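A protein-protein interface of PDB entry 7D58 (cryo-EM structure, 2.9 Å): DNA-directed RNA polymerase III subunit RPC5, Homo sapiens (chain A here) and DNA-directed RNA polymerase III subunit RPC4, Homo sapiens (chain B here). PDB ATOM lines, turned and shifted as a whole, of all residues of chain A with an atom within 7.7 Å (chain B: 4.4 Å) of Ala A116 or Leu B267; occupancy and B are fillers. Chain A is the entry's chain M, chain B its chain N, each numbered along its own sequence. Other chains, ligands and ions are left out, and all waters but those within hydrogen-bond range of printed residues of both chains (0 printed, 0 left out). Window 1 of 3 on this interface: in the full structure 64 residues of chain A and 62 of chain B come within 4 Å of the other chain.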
ATOM      1  N   TYR A  16      -3.661 -16.458   3.559  1.00  0.00           N
ATOM      2  CA  TYR A  16      -2.659 -17.504   3.686  1.00  0.00           C
ATOM      3  C   TYR A  16      -2.032 -17.456   5.074  1.00  0.00           C
ATOM      4  O   TYR A  16      -2.020 -16.415   5.737  1.00  0.00           O
ATOM      5  CB  TYR A  16      -1.557 -17.368   2.626  1.00  0.00           C
ATOM      6  CG  TYR A  16      -2.028 -17.514   1.197  1.00  0.00           C
ATOM      7  CD1 TYR A  16      -2.227 -18.770   0.635  1.00  0.00           C
ATOM      8  CD2 TYR A  16      -2.256 -16.399   0.404  1.00  0.00           C
ATOM      9  CE1 TYR A  16      -2.651 -18.906  -0.674  1.00  0.00           C
ATOM     10  CE2 TYR A  16      -2.677 -16.525  -0.904  1.00  0.00           C
ATOM     11  CZ  TYR A  16      -2.874 -17.781  -1.438  1.00  0.00           C
ATOM     12  OH  TYR A  16      -3.295 -17.910  -2.741  1.00  0.00           O
ATOM     13  N   LEU A  25       9.880 -14.856  15.688  1.00  0.00           N
ATOM     14  CA  LEU A  25       9.059 -13.655  15.563  1.00  0.00           C
ATOM     15  C   LEU A  25       8.720 -13.144  16.953  1.00  0.00           C
ATOM     16  O   LEU A  25       8.191 -13.895  17.778  1.00  0.00           O
ATOM     17  CB  LEU A  25       7.783 -13.942  14.768  1.00  0.00           C
ATOM     18  CG  LEU A  25       7.102 -12.742  14.108  1.00  0.00           C
ATOM     19  CD1 LEU A  25       8.028 -12.088  13.094  1.00  0.00           C
ATOM     20  CD2 LEU A  25       5.797 -13.164  13.451  1.00  0.00           C
ATOM     21  N   LEU A  27       7.100  -9.434  18.774  1.00  0.00           N
ATOM     22  CA  LEU A  27       6.517  -8.114  18.582  1.00  0.00           C
ATOM     23  C   LEU A  27       6.939  -7.201  19.726  1.00  0.00           C
ATOM     24  O   LEU A  27       6.679  -7.503  20.895  1.00  0.00           O
ATOM     25  CB  LEU A  27       4.992  -8.198  18.503  1.00  0.00           C
ATOM     26  CG  LEU A  27       4.246  -6.869  18.357  1.00  0.00           C
ATOM     27  CD1 LEU A  27       4.216  -6.425  16.904  1.00  0.00           C
ATOM     28  CD2 LEU A  27       2.836  -6.984  18.916  1.00  0.00           C
ATOM     29  N   ARG A 113      -3.578 -16.557  19.912  1.00  0.00           N
ATOM     30  CA  ARG A 113      -4.562 -15.804  19.143  1.00  0.00           C
ATOM     31  C   ARG A 113      -3.885 -14.761  18.262  1.00  0.00           C
ATOM     32  O   ARG A 113      -4.133 -14.692  17.053  1.00  0.00           O
ATOM     33  CB  ARG A 113      -5.564 -15.138  20.086  1.00  0.00           C
ATOM     34  CG  ARG A 113      -6.133 -16.048  21.166  1.00  0.00           C
ATOM     35  CD  ARG A 113      -6.945 -15.240  22.176  1.00  0.00           C
ATOM     36  NE  ARG A 113      -7.688 -16.091  23.101  1.00  0.00           N
ATOM     37  CZ  ARG A 113      -7.249 -16.452  24.304  1.00  0.00           C
ATOM     38  NH1 ARG A 113      -7.994 -17.231  25.079  1.00  0.00           N
ATOM     39  NH2 ARG A 113      -6.068 -16.032  24.735  1.00  0.00           N
ATOM     40  N   TYR A 114      -3.021 -13.940  18.856  1.00  0.00           N
ATOM     41  CA  TYR A 114      -2.397 -12.829  18.150  1.00  0.00           C
ATOM     42  C   TYR A 114      -1.490 -13.317  17.029  1.00  0.00           C
ATOM     43  O   TYR A 114      -0.593 -14.136  17.251  1.00  0.00           O
ATOM     44  CB  TYR A 114      -1.607 -11.976  19.144  1.00  0.00           C
ATOM     45  CG  TYR A 114      -2.386 -11.606  20.388  1.00  0.00           C
ATOM     46  CD1 TYR A 114      -3.453 -10.719  20.326  1.00  0.00           C
ATOM     47  CD2 TYR A 114      -2.052 -12.141  21.625  1.00  0.00           C
ATOM     48  CE1 TYR A 114      -4.166 -10.378  21.459  1.00  0.00           C
ATOM     49  CE2 TYR A 114      -2.758 -11.805  22.764  1.00  0.00           C
ATOM     50  CZ  TYR A 114      -3.814 -10.924  22.675  1.00  0.00           C
ATOM     51  OH  TYR A 114      -4.522 -10.585  23.805  1.00  0.00           O
ATOM     52  N   ALA A 115      -1.725 -12.805  15.821  1.00  0.00           N
ATOM     53  CA  ALA A 115      -0.926 -13.143  14.653  1.00  0.00           C
ATOM     54  C   ALA A 115      -0.741 -11.901  13.794  1.00  0.00           C
ATOM     55  O   ALA A 115      -1.651 -11.075  13.683  1.00  0.00           O
ATOM     56  CB  ALA A 115      -1.576 -14.261  13.830  1.00  0.00           C
ATOM     57  N   ALA A 116       0.436 -11.775  13.187  1.00  0.00           N
ATOM     58  CA  ALA A 116       0.734 -10.620  12.352  1.00  0.00           C
ATOM     59  C   ALA A 116       0.189 -10.823  10.945  1.00  0.00           C
ATOM     60  O   ALA A 116       0.234 -11.928  10.400  1.00  0.00           O
ATOM     61  CB  ALA A 116       2.242 -10.370  12.300  1.00  0.00           C
ATOM     62  N   ALA A 117      -0.324  -9.747  10.353  1.00  0.00           N
ATOM     63  CA  ALA A 117      -0.956  -9.801   9.043  1.00  0.00           C
ATOM     64  C   ALA A 117      -0.283  -8.823   8.090  1.00  0.00           C
ATOM     65  O   ALA A 117      -0.088  -7.651   8.424  1.00  0.00           O
ATOM     66  CB  ALA A 117      -2.453  -9.486   9.141  1.00  0.00           C
ATOM     67  N   LEU A 118       0.071  -9.313   6.906  1.00  0.00           N
ATOM     68  CA  LEU A 118       0.643  -8.498   5.842  1.00  0.00           C
ATOM     69  C   LEU A 118      -0.302  -8.514   4.651  1.00  0.00           C
ATOM     70  O   LEU A 118      -0.785  -9.578   4.250  1.00  0.00           O
ATOM     71  CB  LEU A 118       2.035  -9.004   5.441  1.00  0.00           C
ATOM     72  CG  LEU A 118       2.856  -8.158   4.460  1.00  0.00           C
ATOM     73  CD1 LEU A 118       4.339  -8.303   4.752  1.00  0.00           C
ATOM     74  CD2 LEU A 118       2.574  -8.553   3.015  1.00  0.00           C
ATOM     75  N   TYR A 119      -0.559  -7.337   4.087  1.00  0.00           N
ATOM     76  CA  TYR A 119      -1.497  -7.168   2.980  1.00  0.00           C
ATOM     77  C   TYR A 119      -0.710  -6.764   1.737  1.00  0.00           C
ATOM     78  O   TYR A 119      -0.249  -5.624   1.625  1.00  0.00           O
ATOM     79  CB  TYR A 119      -2.562  -6.132   3.329  1.00  0.00           C
ATOM     80  CG  TYR A 119      -3.639  -5.970   2.280  1.00  0.00           C
ATOM     81  CD1 TYR A 119      -4.462  -7.033   1.934  1.00  0.00           C
ATOM     82  CD2 TYR A 119      -3.838  -4.753   1.642  1.00  0.00           C
ATOM     83  CE1 TYR A 119      -5.450  -6.891   0.978  1.00  0.00           C
ATOM     84  CE2 TYR A 119      -4.824  -4.600   0.684  1.00  0.00           C
ATOM     85  CZ  TYR A 119      -5.627  -5.673   0.356  1.00  0.00           C
ATOM     86  OH  TYR A 119      -6.609  -5.528  -0.595  1.00  0.00           O
ATOM     87  N   LEU A 124      -3.557 -11.802   1.601  1.00  0.00           N
ATOM     88  CA  LEU A 124      -3.246 -11.536   2.999  1.00  0.00           C
ATOM     89  C   LEU A 124      -2.485 -12.716   3.582  1.00  0.00           C
ATOM     90  O   LEU A 124      -2.897 -13.870   3.416  1.00  0.00           O
ATOM     91  CB  LEU A 124      -4.524 -11.284   3.804  1.00  0.00           C
ATOM     92  CG  LEU A 124      -4.948  -9.831   4.027  1.00  0.00           C
ATOM     93  CD1 LEU A 124      -6.389  -9.765   4.512  1.00  0.00           C
ATOM     94  CD2 LEU A 124      -4.018  -9.141   5.014  1.00  0.00           C
ATOM     95  N   HIS A 125      -1.378 -12.430   4.261  1.00  0.00           N
ATOM     96  CA  HIS A 125      -0.573 -13.454   4.907  1.00  0.00           C
ATOM     97  C   HIS A 125      -0.566 -13.248   6.416  1.00  0.00           C
ATOM     98  O   HIS A 125      -0.185 -12.185   6.914  1.00  0.00           O
ATOM     99  CB  HIS A 125       0.862 -13.449   4.372  1.00  0.00           C
ATOM    100  CG  HIS A 125       0.959 -13.729   2.905  1.00  0.00           C
ATOM    101  ND1 HIS A 125       1.178 -12.739   1.972  1.00  0.00           N
ATOM    102  CD2 HIS A 125       0.863 -14.886   2.210  1.00  0.00           C
ATOM    103  CE1 HIS A 125       1.216 -13.275   0.765  1.00  0.00           C
ATOM    104  NE2 HIS A 125       1.027 -14.578   0.882  1.00  0.00           N
ATOM    105  N   LEU A 126      -0.980 -14.284   7.142  1.00  0.00           N
ATOM    106  CA  LEU A 126      -1.043 -14.248   8.599  1.00  0.00           C
ATOM    107  C   LEU A 126      -0.012 -15.212   9.162  1.00  0.00           C
ATOM    108  O   LEU A 126      -0.039 -16.407   8.854  1.00  0.00           O
ATOM    109  CB  LEU A 126      -2.445 -14.603   9.108  1.00  0.00           C
ATOM    110  CG  LEU A 126      -3.496 -13.489   9.149  1.00  0.00           C
ATOM    111  CD1 LEU A 126      -3.965 -13.102   7.757  1.00  0.00           C
ATOM    112  CD2 LEU A 126      -4.678 -13.895  10.021  1.00  0.00           C
ATOM    113  N   THR A 127       0.883 -14.692   9.993  1.00  0.00           N
ATOM    114  CA  THR A 127       1.925 -15.494  10.626  1.00  0.00           C
ATOM    115  C   THR A 127       1.718 -15.496  12.132  1.00  0.00           C
ATOM    116  O   THR A 127       1.581 -14.418  12.735  1.00  0.00           O
ATOM    117  CB  THR A 127       3.313 -14.955  10.277  1.00  0.00           C
ATOM    118  OG1 THR A 127       3.408 -14.750   8.863  1.00  0.00           O
ATOM    119  CG2 THR A 127       4.388 -15.940  10.712  1.00  0.00           C
ATOM    120  N   PRO A 128       1.672 -16.661  12.775  1.00  0.00           N
ATOM    121  CA  PRO A 128       1.467 -16.700  14.229  1.00  0.00           C
ATOM    122  C   PRO A 128       2.616 -16.043  14.977  1.00  0.00           C
ATOM    123  O   PRO A 128       3.781 -16.146  14.584  1.00  0.00           O
ATOM    124  CB  PRO A 128       1.381 -18.200  14.532  1.00  0.00           C
ATOM    125  CG  PRO A 128       1.040 -18.845  13.228  1.00  0.00           C
ATOM    126  CD  PRO A 128       1.703 -18.007  12.182  1.00  0.00           C
ATOM    127  N   LEU A 129       2.280 -15.368  16.073  1.00  0.00           N
ATOM    128  CA  LEU A 129       3.270 -14.690  16.896  1.00  0.00           C
ATOM    129  C   LEU A 129       3.704 -15.579  18.053  1.00  0.00           C
ATOM    130  O   LEU A 129       2.880 -16.256  18.677  1.00  0.00           O
ATOM    131  CB  LEU A 129       2.710 -13.371  17.433  1.00  0.00           C
ATOM    132  CG  LEU A 129       3.052 -12.115  16.629  1.00  0.00           C
ATOM    133  CD1 LEU A 129       2.272 -10.920  17.149  1.00  0.00           C
ATOM    134  CD2 LEU A 129       4.545 -11.840  16.680  1.00  0.00           C
ATOM    135  N   LEU A 225       8.440 -14.600   4.990  1.00  0.00           N
ATOM    136  CA  LEU A 225       7.138 -14.486   5.633  1.00  0.00           C
ATOM    137  C   LEU A 225       6.018 -14.205   4.640  1.00  0.00           C
ATOM    138  O   LEU A 225       4.844 -14.353   4.993  1.00  0.00           O
ATOM    139  CB  LEU A 225       7.165 -13.396   6.715  1.00  0.00           C
ATOM    140  CG  LEU A 225       7.306 -11.922   6.322  1.00  0.00           C
ATOM    141  CD1 LEU A 225       5.944 -11.260   6.160  1.00  0.00           C
ATOM    142  CD2 LEU A 225       8.137 -11.166   7.348  1.00  0.00           C
ATOM    143  N   GLU B 265       1.716  -2.921   3.866  1.00  0.00           N
ATOM    144  CA  GLU B 265       1.936  -2.632   5.275  1.00  0.00           C
ATOM    145  C   GLU B 265       1.481  -3.821   6.109  1.00  0.00           C
ATOM    146  O   GLU B 265       0.695  -4.659   5.661  1.00  0.00           O
ATOM    147  CB  GLU B 265       1.198  -1.360   5.715  1.00  0.00           C
ATOM    148  CG  GLU B 265      -0.312  -1.505   5.772  1.00  0.00           C
ATOM    149  CD  GLU B 265      -1.013  -0.179   5.985  1.00  0.00           C
ATOM    150  OE1 GLU B 265      -0.706   0.782   5.247  1.00  0.00           O
ATOM    151  OE2 GLU B 265      -1.870  -0.096   6.890  1.00  0.00           O
ATOM    152  N   LEU B 266       1.992  -3.885   7.335  1.00  0.00           N
ATOM    153  CA  LEU B 266       1.686  -4.980   8.242  1.00  0.00           C
ATOM    154  C   LEU B 266       0.524  -4.613   9.158  1.00  0.00           C
ATOM    155  O   LEU B 266       0.304  -3.441   9.477  1.00  0.00           O
ATOM    156  CB  LEU B 266       2.916  -5.352   9.074  1.00  0.00           C
ATOM    157  CG  LEU B 266       3.964  -6.233   8.385  1.00  0.00           C
ATOM    158  CD1 LEU B 266       4.856  -5.416   7.459  1.00  0.00           C
ATOM    159  CD2 LEU B 266       4.800  -6.984   9.407  1.00  0.00           C
ATOM    160  N   LEU B 267      -0.220  -5.634   9.579  1.00  0.00           N
ATOM    161  CA  LEU B 267      -1.396  -5.464  10.423  1.00  0.00           C
ATOM    162  C   LEU B 267      -1.339  -6.465  11.568  1.00  0.00           C
ATOM    163  O   LEU B 267      -0.844  -7.583  11.395  1.00  0.00           O
ATOM    164  CB  LEU B 267      -2.688  -5.655   9.620  1.00  0.00           C
ATOM    165  CG  LEU B 267      -2.927  -4.705   8.443  1.00  0.00           C
ATOM    166  CD1 LEU B 267      -4.175  -5.108   7.672  1.00  0.00           C
ATOM    167  CD2 LEU B 267      -3.029  -3.266   8.923  1.00  0.00           C
ATOM    168  N   PHE B 268      -1.840  -6.062  12.733  1.00  0.00           N
ATOM    169  CA  PHE B 268      -1.879  -6.918  13.914  1.00  0.00           C
ATOM    170  C   PHE B 268      -3.324  -7.344  14.151  1.00  0.00           C
ATOM    171  O   PHE B 268      -4.180  -6.513  14.471  1.00  0.00           O
ATOM    172  CB  PHE B 268      -1.305  -6.189  15.127  1.00  0.00           C
ATOM    173  CG  PHE B 268      -1.308  -7.004  16.385  1.00  0.00           C
ATOM    174  CD1 PHE B 268      -0.664  -8.227  16.432  1.00  0.00           C
ATOM    175  CD2 PHE B 268      -1.931  -6.536  17.528  1.00  0.00           C
ATOM    176  CE1 PHE B 268      -0.660  -8.976  17.590  1.00  0.00           C
ATOM    177  CE2 PHE B 268      -1.929  -7.280  18.691  1.00  0.00           C
ATOM    178  CZ  PHE B 268      -1.291  -8.502  18.722  1.00  0.00           C
ATOM    179  N   LEU B 269      -3.594  -8.638  13.997  1.00  0.00           N
ATOM    180  CA  LEU B 269      -4.946  -9.163  14.100  1.00  0.00           C
ATOM    181  C   LEU B 269      -5.040 -10.131  15.271  1.00  0.00           C
ATOM    182  O   LEU B 269      -4.109 -10.885  15.561  1.00  0.00           O
ATOM    183  CB  LEU B 269      -5.373  -9.864  12.801  1.00  0.00           C
ATOM    184  CG  LEU B 269      -6.222  -9.049  11.821  1.00  0.00           C
ATOM    185  CD1 LEU B 269      -5.455  -7.842  11.308  1.00  0.00           C
ATOM    186  CD2 LEU B 269      -6.679  -9.920  10.663  1.00  0.00           C
ATOM    187  N   LEU B 360       7.739  -5.041  14.764  1.00  0.00           N
ATOM    188  CA  LEU B 360       8.086  -6.443  14.952  1.00  0.00           C
ATOM    189  C   LEU B 360       9.399  -6.751  14.244  1.00  0.00           C
ATOM    190  O   LEU B 360       9.607  -6.335  13.100  1.00  0.00           O
ATOM    191  CB  LEU B 360       6.963  -7.363  14.457  1.00  0.00           C
ATOM    192  CG  LEU B 360       6.473  -7.347  13.005  1.00  0.00           C
ATOM    193  CD1 LEU B 360       7.288  -8.276  12.112  1.00  0.00           C
ATOM    194  CD2 LEU B 360       4.994  -7.707  12.951  1.00  0.00           C
ATOM    195  N   VAL B 379       3.782  -1.768  12.959  1.00  0.00           N
ATOM    196  CA  VAL B 379       2.347  -2.020  12.927  1.00  0.00           C
ATOM    197  C   VAL B 379       1.650  -0.778  13.464  1.00  0.00           C
ATOM    198  O   VAL B 379       2.077  -0.210  14.477  1.00  0.00           O
ATOM    199  CB  VAL B 379       1.964  -3.265  13.740  1.00  0.00           C
ATOM    200  CG1 VAL B 379       0.458  -3.458  13.738  1.00  0.00           C
ATOM    201  CG2 VAL B 379       2.661  -4.495  13.181  1.00  0.00           C
ATOM    202  N   HIS B 381      -2.109  -0.620  13.106  1.00  0.00           N
ATOM    203  CA  HIS B 381      -3.538  -0.923  13.066  1.00  0.00           C
ATOM    204  C   HIS B 381      -3.754  -2.275  13.730  1.00  0.00           C
ATOM    205  O   HIS B 381      -3.061  -3.243  13.402  1.00  0.00           O
ATOM    206  CB  HIS B 381      -4.063  -0.931  11.632  1.00  0.00           C
ATOM    207  CG  HIS B 381      -4.327   0.433  11.077  1.00  0.00           C
ATOM    208  ND1 HIS B 381      -5.235   1.304  11.641  1.00  0.00           N
ATOM    209  CD2 HIS B 381      -3.809   1.076  10.003  1.00  0.00           C
ATOM    210  CE1 HIS B 381      -5.261   2.425  10.942  1.00  0.00           C
ATOM    211  NE2 HIS B 381      -4.405   2.312   9.942  1.00  0.00           N
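O of Ala A116 lies within hydrogen-bond range of N of Thr A127, 2.9 Å away.
The backbone NH of Phe B268 lies within hydrogen-bond range of the backbone carbonyl oxygen of His B381 (3.1 Å).
The backbone NH of Leu A118 is in hydrogen-bond range of the backbone carbonyl oxygen of His A125, at 2.9 Å.
O of Tyr A114 lies within hydrogen-bond range of N of Leu A129 (3.3 Å).
The backbone NH (N) of Tyr A119 sits at hydrogen-bond distance from the backbone carbonyl oxygen (O) of Glu B265.
The backbone carbonyl oxygen (O) of Leu B269 sits at hydrogen-bond distance from the backbone NH (N) of Ala A115 (3.1 Å).
N of Ala A117 lies within hydrogen-bond range of O of Leu B267 (2.5 Å).
CB of Leu B360 touches CD1 of Leu A27, at 3.8 Å.
Tyr A114 touches Phe B268 (CD1 to CZ, 3.5 Å).
Tyr A114 touches Leu B269.
O of Leu B267 touches C of Ala A116, 3.4 Å away.
CD2 of Leu B360 touches CB of Ala A116 (3.9 Å).
C of Leu B266 touches O of Ala A117, at 3.2 Å.
CA of Leu A118 touches O of Glu B265, 3.8 Å away.
Leu A118 touches Leu B266.
Phe B268 touches Leu A129.
Leu B267 touches just these residues of chain A: Ala A116 and Ala A117.
Printed residues of chain A within 4 Å of Leu B269: Tyr A114 (3.7 Å) and Ala A115 (3.1 Å).
Of the printed residues of chain A, Phe B268 touches Tyr A114 (3.5 Å) and Leu A129 (3.5 Å).
Of the printed residues of chain B, Leu A129 touches Phe B268.
Of the printed residues of chain A, Leu B266 touches Ala A117 and Leu A118.
Leu A124 touches none of the printed residues of chain B.
The nearest printed residue of chain B that does not touch Ala A116 is Phe B268 (4.8 Å).
The nearest printed residue of chain B that does not touch Tyr A119 is Leu B267 (4.7 Å).
Hydrophobic or aromatic side chains of chain A that line the printed part of chain B: Leu A27, Tyr A114, Ala A116, Ala A117, Leu A118 and Leu A129.
Hydrophobic or aromatic side chains of chain B that line the printed part of chain A: Leu B266, Leu B267, Phe B268 and Leu B360.
Among the printed residues, no Asp or Glu carboxylate lies within 4 Å of a Lys or Arg side-chain nitrogen of the other chain.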
